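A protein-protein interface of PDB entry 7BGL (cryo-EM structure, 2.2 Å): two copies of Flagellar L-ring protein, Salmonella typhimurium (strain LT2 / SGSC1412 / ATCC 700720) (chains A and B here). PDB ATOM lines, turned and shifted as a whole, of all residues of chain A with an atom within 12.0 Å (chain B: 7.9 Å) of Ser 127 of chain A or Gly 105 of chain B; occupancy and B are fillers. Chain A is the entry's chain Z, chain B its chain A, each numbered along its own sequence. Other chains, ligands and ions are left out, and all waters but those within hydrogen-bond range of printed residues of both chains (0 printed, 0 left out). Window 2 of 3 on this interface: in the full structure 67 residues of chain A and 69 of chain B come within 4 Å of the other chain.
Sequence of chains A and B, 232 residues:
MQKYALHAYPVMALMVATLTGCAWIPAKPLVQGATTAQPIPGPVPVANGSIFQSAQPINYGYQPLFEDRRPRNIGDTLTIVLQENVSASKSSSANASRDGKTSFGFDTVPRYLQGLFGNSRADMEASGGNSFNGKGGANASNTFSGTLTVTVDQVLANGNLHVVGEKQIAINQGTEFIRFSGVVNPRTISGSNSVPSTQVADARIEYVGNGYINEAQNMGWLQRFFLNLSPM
The backbone NH (N) of Ser 103 of chain B is in hydrogen-bond range of the backbone carbonyl oxygen (O) of Gly 129 of chain A, 2.8 Å away. The backbone carbonyl oxygen (O) of Gly 105 of chain B lies within hydrogen-bond range of the backbone NH (N) of Ser 127 of chain A (2.8 Å). The backbone carbonyl oxygen of Phe 106 of chain B sits close to the backbone carbonyl oxygen of Glu 125 of chain A. The backbone carbonyl oxygen (O) of Thr 108 of chain B sits at hydrogen-bond distance from the backbone NH (N) of Glu 125 of chain A.
N of Phe 104 of chain B lies within hydrogen-bond range of O of Met 124 of chain B. The backbone NH of Gly 128 of chain A is in hydrogen-bond range of the backbone carbonyl oxygen of Gly 100 of chain A (2.9 Å). The backbone carbonyl oxygen (O) of Ala 126 of chain A sits at hydrogen-bond distance from the backbone NH (N) of Thr 102 of chain A, 2.9 Å away.
Asp 123 of chain A touches Thr 108 of chain B. C of Val 109 of chain B touches O of Asp 123 of chain A, 3.8 Å away. CA of Ala 126 of chain A touches O of Gly 105 of chain B (3.4 Å). O of Phe 106 of chain B touches N of Ala 126 of chain A (3.7 Å). Ser 127 of chain A touches Phe 104 of chain B. CA of Gly 128 of chain A touches O of Ser 103 of chain B (3.4 Å).
Of the printed residues of chain B, Glu 125 of chain A touches Phe 106 and Thr 108. Ala 126 of chain A touches just these residues of chain B: Gly 105 and Phe 106. Of chain B, only Phe 104 (3.0 Å) and Gly 105 (2.8 Å) come within 4 Å of Ser 127 of chain A. Printed residues of chain B within 4 Å of Gly 128 of chain A: Ser 103. Printed residues of chain B within 4 Å of Gly 129 of chain A: Ser 103. Of chain A, only Gly 128 (3.4 Å) and Gly 129 (2.8 Å) come within 4 Å of Ser 103 of chain B. Phe 104 of chain B touches just one residue of chain A: Ser 127. Gly 105 of chain B touches just these residues of chain A: Ala 126 (3.4 Å) and Ser 127 (2.8 Å). No residue of chain A comes within 4 Å of Asp 107 of chain B. Ala 122 of chain B touches none of the printed residues of chain A. No residue of chain A comes within 4 Å of Asp 123 of chain B. The nearest printed residue of chain B that does not touch Gly 128 of chain A is Phe 104 of chain B (4.1 Å).
Of the 13 printed residues of chain B, 6 touch a printed residue of chain A. Hydrophobic or aromatic side chains of chain B that line the printed part of chain A: Phe 104 and Phe 106. Of the 16 printed residues of chain A, 6 touch a printed residue of chain B. Among the printed residues, no Asp or Glu carboxylate lies within 4 Å of a Lys or Arg side-chain nitrogen of the other chain.
Positions printed for both chains: 103, 104, 123, 124 and 125. Of the 10 pairs that touch across the chains among the printed residues, none has its exchanged pair printed and touching as well.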
ATOM      1  N   ARG A  98      -5.507   1.310  17.399  1.00  0.00           N
ATOM      2  CA  ARG A  98      -5.328   0.427  16.257  1.00  0.00           C
ATOM      3  C   ARG A  98      -6.436  -0.613  16.272  1.00  0.00           C
ATOM      4  O   ARG A  98      -6.697  -1.231  17.309  1.00  0.00           O
ATOM      5  CB  ARG A  98      -3.960  -0.255  16.281  1.00  0.00           C
ATOM      6  CG  ARG A  98      -3.621  -0.976  14.990  1.00  0.00           C
ATOM      7  CD  ARG A  98      -2.199  -1.500  14.987  1.00  0.00           C
ATOM      8  NE  ARG A  98      -2.093  -2.791  15.654  1.00  0.00           N
ATOM      9  CZ  ARG A  98      -0.948  -3.414  15.902  1.00  0.00           C
ATOM     10  NH1 ARG A  98       0.213  -2.893  15.541  1.00  0.00           N
ATOM     11  NH2 ARG A  98      -0.971  -4.587  16.525  1.00  0.00           N
ATOM     12  N   ASP A  99      -7.089  -0.798  15.130  1.00  0.00           N
ATOM     13  CA  ASP A  99      -8.155  -1.782  15.008  1.00  0.00           C
ATOM     14  C   ASP A  99      -8.013  -2.509  13.682  1.00  0.00           C
ATOM     15  O   ASP A  99      -7.840  -1.875  12.638  1.00  0.00           O
ATOM     16  CB  ASP A  99      -9.537  -1.124  15.104  1.00  0.00           C
ATOM     17  CG  ASP A  99     -10.012  -0.970  16.534  1.00  0.00           C
ATOM     18  OD1 ASP A  99     -11.045  -1.576  16.885  1.00  0.00           O
ATOM     19  OD2 ASP A  99      -9.349  -0.249  17.310  1.00  0.00           O
ATOM     20  N   GLY A 100      -8.091  -3.830  13.729  1.00  0.00           N
ATOM     21  CA  GLY A 100      -8.056  -4.635  12.523  1.00  0.00           C
ATOM     22  C   GLY A 100      -9.002  -5.803  12.664  1.00  0.00           C
ATOM     23  O   GLY A 100      -9.269  -6.283  13.767  1.00  0.00           O
ATOM     24  N   LYS A 101      -9.533  -6.249  11.532  1.00  0.00           N
ATOM     25  CA  LYS A 101     -10.503  -7.337  11.553  1.00  0.00           C
ATOM     26  C   LYS A 101     -10.636  -7.916  10.155  1.00  0.00           C
ATOM     27  O   LYS A 101     -11.134  -7.241   9.250  1.00  0.00           O
ATOM     28  CB  LYS A 101     -11.850  -6.841  12.084  1.00  0.00           C
ATOM     29  CG  LYS A 101     -12.990  -7.824  11.971  1.00  0.00           C
ATOM     30  CD  LYS A 101     -14.322  -7.102  12.019  1.00  0.00           C
ATOM     31  CE  LYS A 101     -14.722  -6.621  10.637  1.00  0.00           C
ATOM     32  NZ  LYS A 101     -13.591  -6.732   9.680  1.00  0.00           N
ATOM     33  N   THR A 102     -10.198  -9.161   9.990  1.00  0.00           N
ATOM     34  CA  THR A 102     -10.126  -9.817   8.695  1.00  0.00           C
ATOM     35  C   THR A 102     -11.032 -11.039   8.670  1.00  0.00           C
ATOM     36  O   THR A 102     -11.249 -11.685   9.702  1.00  0.00           O
ATOM     37  CB  THR A 102      -8.691 -10.237   8.375  1.00  0.00           C
ATOM     38  OG1 THR A 102      -8.261 -11.225   9.318  1.00  0.00           O
ATOM     39  CG2 THR A 102      -7.763  -9.042   8.466  1.00  0.00           C
ATOM     40  N   SER A 103     -11.564 -11.344   7.489  1.00  0.00           N
ATOM     41  CA  SER A 103     -12.471 -12.468   7.319  1.00  0.00           C
ATOM     42  C   SER A 103     -12.280 -13.071   5.936  1.00  0.00           C
ATOM     43  O   SER A 103     -11.825 -12.403   5.006  1.00  0.00           O
ATOM     44  CB  SER A 103     -13.929 -12.041   7.514  1.00  0.00           C
ATOM     45  OG  SER A 103     -14.816 -13.115   7.253  1.00  0.00           O
ATOM     46  N   PHE A 104     -12.631 -14.351   5.817  1.00  0.00           N
ATOM     47  CA  PHE A 104     -12.622 -15.058   4.542  1.00  0.00           C
ATOM     48  C   PHE A 104     -13.389 -16.366   4.662  1.00  0.00           C
ATOM     49  O   PHE A 104     -13.131 -17.158   5.572  1.00  0.00           O
ATOM     50  CB  PHE A 104     -11.194 -15.334   4.073  1.00  0.00           C
ATOM     51  CG  PHE A 104     -11.121 -16.215   2.858  1.00  0.00           C
ATOM     52  CD1 PHE A 104     -11.695 -15.818   1.664  1.00  0.00           C
ATOM     53  CD2 PHE A 104     -10.500 -17.449   2.919  1.00  0.00           C
ATOM     54  CE1 PHE A 104     -11.640 -16.629   0.548  1.00  0.00           C
ATOM     55  CE2 PHE A 104     -10.442 -18.265   1.807  1.00  0.00           C
ATOM     56  CZ  PHE A 104     -11.011 -17.855   0.621  1.00  0.00           C
ATOM     57  N   ASP A 123     -11.166 -21.223   5.691  1.00  0.00           N
ATOM     58  CA  ASP A 123     -12.055 -20.290   6.369  1.00  0.00           C
ATOM     59  C   ASP A 123     -11.330 -19.619   7.524  1.00  0.00           C
ATOM     60  O   ASP A 123     -10.829 -20.289   8.431  1.00  0.00           O
ATOM     61  CB  ASP A 123     -13.301 -21.021   6.869  1.00  0.00           C
ATOM     62  CG  ASP A 123     -14.330 -21.229   5.776  1.00  0.00           C
ATOM     63  OD1 ASP A 123     -15.540 -21.212   6.083  1.00  0.00           O
ATOM     64  OD2 ASP A 123     -13.928 -21.412   4.608  1.00  0.00           O
ATOM     65  N   MET A 124     -11.275 -18.292   7.488  1.00  0.00           N
ATOM     66  CA  MET A 124     -10.500 -17.516   8.442  1.00  0.00           C
ATOM     67  C   MET A 124     -11.331 -16.362   8.978  1.00  0.00           C
ATOM     68  O   MET A 124     -12.166 -15.792   8.272  1.00  0.00           O
ATOM     69  CB  MET A 124      -9.214 -16.979   7.803  1.00  0.00           C
ATOM     70  CG  MET A 124      -8.281 -16.278   8.770  1.00  0.00           C
ATOM     71  SD  MET A 124      -8.503 -14.490   8.750  1.00  0.00           S
ATOM     72  CE  MET A 124      -8.574 -14.182   6.987  1.00  0.00           C
ATOM     73  N   GLU A 125     -11.084 -16.019  10.239  1.00  0.00           N
ATOM     74  CA  GLU A 125     -11.746 -14.894  10.884  1.00  0.00           C
ATOM     75  C   GLU A 125     -10.888 -14.457  12.058  1.00  0.00           C
ATOM     76  O   GLU A 125     -10.479 -15.293  12.867  1.00  0.00           O
ATOM     77  CB  GLU A 125     -13.153 -15.275  11.355  1.00  0.00           C
ATOM     78  CG  GLU A 125     -13.877 -14.171  12.099  1.00  0.00           C
ATOM     79  CD  GLU A 125     -14.945 -13.508  11.258  1.00  0.00           C
ATOM     80  OE1 GLU A 125     -14.830 -12.293  10.994  1.00  0.00           O
ATOM     81  OE2 GLU A 125     -15.904 -14.203  10.860  1.00  0.00           O
ATOM     82  N   ALA A 126     -10.608 -13.159  12.145  1.00  0.00           N
ATOM     83  CA  ALA A 126      -9.747 -12.662  13.207  1.00  0.00           C
ATOM     84  C   ALA A 126     -10.061 -11.197  13.462  1.00  0.00           C
ATOM     85  O   ALA A 126     -10.457 -10.475  12.547  1.00  0.00           O
ATOM     86  CB  ALA A 126      -8.267 -12.835  12.851  1.00  0.00           C
ATOM     87  N   SER A 127      -9.887 -10.775  14.712  1.00  0.00           N
ATOM     88  CA  SER A 127     -10.077  -9.386  15.100  1.00  0.00           C
ATOM     89  C   SER A 127      -9.032  -9.013  16.139  1.00  0.00           C
ATOM     90  O   SER A 127      -8.558  -9.860  16.898  1.00  0.00           O
ATOM     91  CB  SER A 127     -11.485  -9.140  15.657  1.00  0.00           C
ATOM     92  OG  SER A 127     -12.474  -9.411  14.680  1.00  0.00           O
ATOM     93  N   GLY A 128      -8.677  -7.732  16.163  1.00  0.00           N
ATOM     94  CA  GLY A 128      -7.700  -7.227  17.103  1.00  0.00           C
ATOM     95  C   GLY A 128      -7.847  -5.741  17.350  1.00  0.00           C
ATOM     96  O   GLY A 128      -8.149  -4.974  16.430  1.00  0.00           O
ATOM     97  N   GLY A 129      -7.635  -5.328  18.591  1.00  0.00           N
ATOM     98  CA  GLY A 129      -7.762  -3.928  18.954  1.00  0.00           C
ATOM     99  C   GLY A 129      -6.739  -3.550  19.998  1.00  0.00           C
ATOM    100  O   GLY A 129      -6.297  -4.385  20.794  1.00  0.00           O
ATOM    101  N   ASN A 130      -6.357  -2.278  19.988  1.00  0.00           N
ATOM    102  CA  ASN A 130      -5.383  -1.755  20.943  1.00  0.00           C
ATOM    103  C   ASN A 130      -5.631  -0.261  21.077  1.00  0.00           C
ATOM    104  O   ASN A 130      -5.317   0.501  20.159  1.00  0.00           O
ATOM    105  CB  ASN A 130      -3.956  -2.036  20.480  1.00  0.00           C
ATOM    106  CG  ASN A 130      -2.977  -2.123  21.630  1.00  0.00           C
ATOM    107  OD1 ASN A 130      -2.971  -1.276  22.521  1.00  0.00           O
ATOM    108  ND2 ASN A 130      -2.140  -3.152  21.617  1.00  0.00           N
ATOM    109  N   SER A 131      -6.195   0.157  22.207  1.00  0.00           N
ATOM    110  CA  SER A 131      -6.527   1.555  22.445  1.00  0.00           C
ATOM    111  C   SER A 131      -5.819   2.039  23.700  1.00  0.00           C
ATOM    112  O   SER A 131      -5.850   1.365  24.734  1.00  0.00           O
ATOM    113  CB  SER A 131      -8.040   1.747  22.581  1.00  0.00           C
ATOM    114  OG  SER A 131      -8.541   1.072  23.722  1.00  0.00           O
ATOM    115  N   SER B 103      -7.250  -6.173  22.750  1.00  0.00           N
ATOM    116  CA  SER B 103      -8.002  -7.387  22.481  1.00  0.00           C
ATOM    117  C   SER B 103      -7.471  -8.047  21.218  1.00  0.00           C
ATOM    118  O   SER B 103      -6.883  -7.390  20.355  1.00  0.00           O
ATOM    119  CB  SER B 103      -9.499  -7.095  22.335  1.00  0.00           C
ATOM    120  OG  SER B 103     -10.217  -8.261  21.976  1.00  0.00           O
ATOM    121  N   PHE B 104      -7.680  -9.359  21.127  1.00  0.00           N
ATOM    122  CA  PHE B 104      -7.339 -10.133  19.939  1.00  0.00           C
ATOM    123  C   PHE B 104      -8.002 -11.501  19.995  1.00  0.00           C
ATOM    124  O   PHE B 104      -7.880 -12.211  20.997  1.00  0.00           O
ATOM    125  CB  PHE B 104      -5.825 -10.295  19.801  1.00  0.00           C
ATOM    126  CG  PHE B 104      -5.421 -11.232  18.698  1.00  0.00           C
ATOM    127  CD1 PHE B 104      -5.756 -10.962  17.384  1.00  0.00           C
ATOM    128  CD2 PHE B 104      -4.727 -12.395  18.981  1.00  0.00           C
ATOM    129  CE1 PHE B 104      -5.395 -11.826  16.370  1.00  0.00           C
ATOM    130  CE2 PHE B 104      -4.363 -13.263  17.971  1.00  0.00           C
ATOM    131  CZ  PHE B 104      -4.697 -12.979  16.664  1.00  0.00           C
ATOM    132  N   GLY B 105      -8.698 -11.883  18.928  1.00  0.00           N
ATOM    133  CA  GLY B 105      -9.367 -13.167  18.892  1.00  0.00           C
ATOM    134  C   GLY B 105      -9.705 -13.630  17.489  1.00  0.00           C
ATOM    135  O   GLY B 105     -10.081 -12.822  16.635  1.00  0.00           O
ATOM    136  N   PHE B 106      -9.577 -14.934  17.238  1.00  0.00           N
ATOM    137  CA  PHE B 106      -9.881 -15.476  15.918  1.00  0.00           C
ATOM    138  C   PHE B 106     -11.370 -15.757  15.753  1.00  0.00           C
ATOM    139  O   PHE B 106     -12.026 -15.184  14.878  1.00  0.00           O
ATOM    140  CB  PHE B 106      -9.068 -16.748  15.668  1.00  0.00           C
ATOM    141  CG  PHE B 106      -7.839 -16.529  14.833  1.00  0.00           C
ATOM    142  CD1 PHE B 106      -6.641 -16.172  15.420  1.00  0.00           C
ATOM    143  CD2 PHE B 106      -7.883 -16.684  13.457  1.00  0.00           C
ATOM    144  CE1 PHE B 106      -5.510 -15.972  14.650  1.00  0.00           C
ATOM    145  CE2 PHE B 106      -6.761 -16.485  12.684  1.00  0.00           C
ATOM    146  CZ  PHE B 106      -5.571 -16.129  13.282  1.00  0.00           C
ATOM    147  N   ASP B 107     -11.917 -16.648  16.578  1.00  0.00           N
ATOM    148  CA  ASP B 107     -13.298 -17.090  16.427  1.00  0.00           C
ATOM    149  C   ASP B 107     -13.440 -18.007  15.217  1.00  0.00           C
ATOM    150  O   ASP B 107     -14.488 -18.629  15.020  1.00  0.00           O
ATOM    151  CB  ASP B 107     -14.242 -15.893  16.301  1.00  0.00           C
ATOM    152  CG  ASP B 107     -14.066 -14.887  17.424  1.00  0.00           C
ATOM    153  OD1 ASP B 107     -12.917 -14.503  17.719  1.00  0.00           O
ATOM    154  OD2 ASP B 107     -15.087 -14.484  18.018  1.00  0.00           O
ATOM    155  N   THR B 108     -12.390 -18.094  14.403  1.00  0.00           N
ATOM    156  CA  THR B 108     -12.323 -19.040  13.296  1.00  0.00           C
ATOM    157  C   THR B 108     -10.875 -19.170  12.843  1.00  0.00           C
ATOM    158  O   THR B 108     -10.255 -18.177  12.449  1.00  0.00           O
ATOM    159  CB  THR B 108     -13.216 -18.598  12.135  1.00  0.00           C
ATOM    160  OG1 THR B 108     -14.576 -18.534  12.572  1.00  0.00           O
ATOM    161  CG2 THR B 108     -13.109 -19.579  10.977  1.00  0.00           C
ATOM    162  N   VAL B 109     -10.325 -20.378  12.896  1.00  0.00           N
ATOM    163  CA  VAL B 109      -8.908 -20.581  12.611  1.00  0.00           C
ATOM    164  C   VAL B 109      -8.759 -21.465  11.380  1.00  0.00           C
ATOM    165  O   VAL B 109      -9.422 -22.508  11.281  1.00  0.00           O
ATOM    166  CB  VAL B 109      -8.181 -21.187  13.820  1.00  0.00           C
ATOM    167  CG1 VAL B 109      -6.677 -21.171  13.597  1.00  0.00           C
ATOM    168  CG2 VAL B 109      -8.545 -20.432  15.087  1.00  0.00           C
ATOM    169  N   PHE B 117      -2.813 -20.956  16.456  1.00  0.00           N
ATOM    170  CA  PHE B 117      -3.997 -20.297  16.997  1.00  0.00           C
ATOM    171  C   PHE B 117      -5.214 -21.215  17.012  1.00  0.00           C
ATOM    172  O   PHE B 117      -6.347 -20.731  17.095  1.00  0.00           O
ATOM    173  CB  PHE B 117      -4.311 -19.027  16.203  1.00  0.00           C
ATOM    174  CG  PHE B 117      -3.092 -18.263  15.770  1.00  0.00           C
ATOM    175  CD1 PHE B 117      -2.533 -17.301  16.592  1.00  0.00           C
ATOM    176  CD2 PHE B 117      -2.506 -18.505  14.540  1.00  0.00           C
ATOM    177  CE1 PHE B 117      -1.415 -16.596  16.198  1.00  0.00           C
ATOM    178  CE2 PHE B 117      -1.387 -17.804  14.140  1.00  0.00           C
ATOM    179  CZ  PHE B 117      -0.840 -16.847  14.970  1.00  0.00           C
ATOM    180  N   SER B 120      -7.606 -21.155  21.989  1.00  0.00           N
ATOM    181  CA  SER B 120      -7.518 -19.771  22.430  1.00  0.00           C
ATOM    182  C   SER B 120      -6.113 -19.395  22.882  1.00  0.00           C
ATOM    183  O   SER B 120      -5.949 -18.419  23.623  1.00  0.00           O
ATOM    184  CB  SER B 120      -8.521 -19.512  23.554  1.00  0.00           C
ATOM    185  OG  SER B 120      -9.828 -19.333  23.038  1.00  0.00           O
ATOM    186  N   ALA B 122      -3.687 -17.925  21.459  1.00  0.00           N
ATOM    187  CA  ALA B 122      -3.363 -16.545  21.131  1.00  0.00           C
ATOM    188  C   ALA B 122      -4.458 -15.566  21.525  1.00  0.00           C
ATOM    189  O   ALA B 122      -4.206 -14.357  21.546  1.00  0.00           O
ATOM    190  CB  ALA B 122      -3.079 -16.410  19.633  1.00  0.00           C
ATOM    191  N   ASP B 123      -5.658 -16.053  21.832  1.00  0.00           N
ATOM    192  CA  ASP B 123      -6.745 -15.173  22.237  1.00  0.00           C
ATOM    193  C   ASP B 123      -6.343 -14.371  23.464  1.00  0.00           C
ATOM    194  O   ASP B 123      -5.996 -14.936  24.504  1.00  0.00           O
ATOM    195  CB  ASP B 123      -8.005 -15.992  22.520  1.00  0.00           C
ATOM    196  CG  ASP B 123      -8.754 -16.361  21.255  1.00  0.00           C
ATOM    197  OD1 ASP B 123      -9.999 -16.444  21.301  1.00  0.00           O
ATOM    198  OD2 ASP B 123      -8.097 -16.570  20.214  1.00  0.00           O
ATOM    199  N   MET B 124      -6.393 -13.048  23.339  1.00  0.00           N
ATOM    200  CA  MET B 124      -5.907 -12.148  24.372  1.00  0.00           C
ATOM    201  C   MET B 124      -6.928 -11.052  24.633  1.00  0.00           C
ATOM    202  O   MET B 124      -7.635 -10.607  23.726  1.00  0.00           O
ATOM    203  CB  MET B 124      -4.564 -11.525  23.975  1.00  0.00           C
ATOM    204  CG  MET B 124      -3.921 -10.683  25.060  1.00  0.00           C
ATOM    205  SD  MET B 124      -4.280  -8.930  24.857  1.00  0.00           S
ATOM    206  CE  MET B 124      -3.998  -8.730  23.101  1.00  0.00           C
ATOM    207  N   GLU B 125      -6.986 -10.615  25.888  1.00  0.00           N
ATOM    208  CA  GLU B 125      -7.863  -9.525  26.292  1.00  0.00           C
ATOM    209  C   GLU B 125      -7.315  -8.941  27.583  1.00  0.00           C
ATOM    210  O   GLU B 125      -7.022  -9.687  28.521  1.00  0.00           O
ATOM    211  CB  GLU B 125      -9.300 -10.013  26.488  1.00  0.00           C
ATOM    212  CG  GLU B 125     -10.256  -8.945  26.977  1.00  0.00           C
ATOM    213  CD  GLU B 125     -11.171  -8.438  25.884  1.00  0.00           C
ATOM    214  OE1 GLU B 125     -11.102  -7.235  25.559  1.00  0.00           O
ATOM    215  OE2 GLU B 125     -11.960  -9.244  25.349  1.00  0.00           O
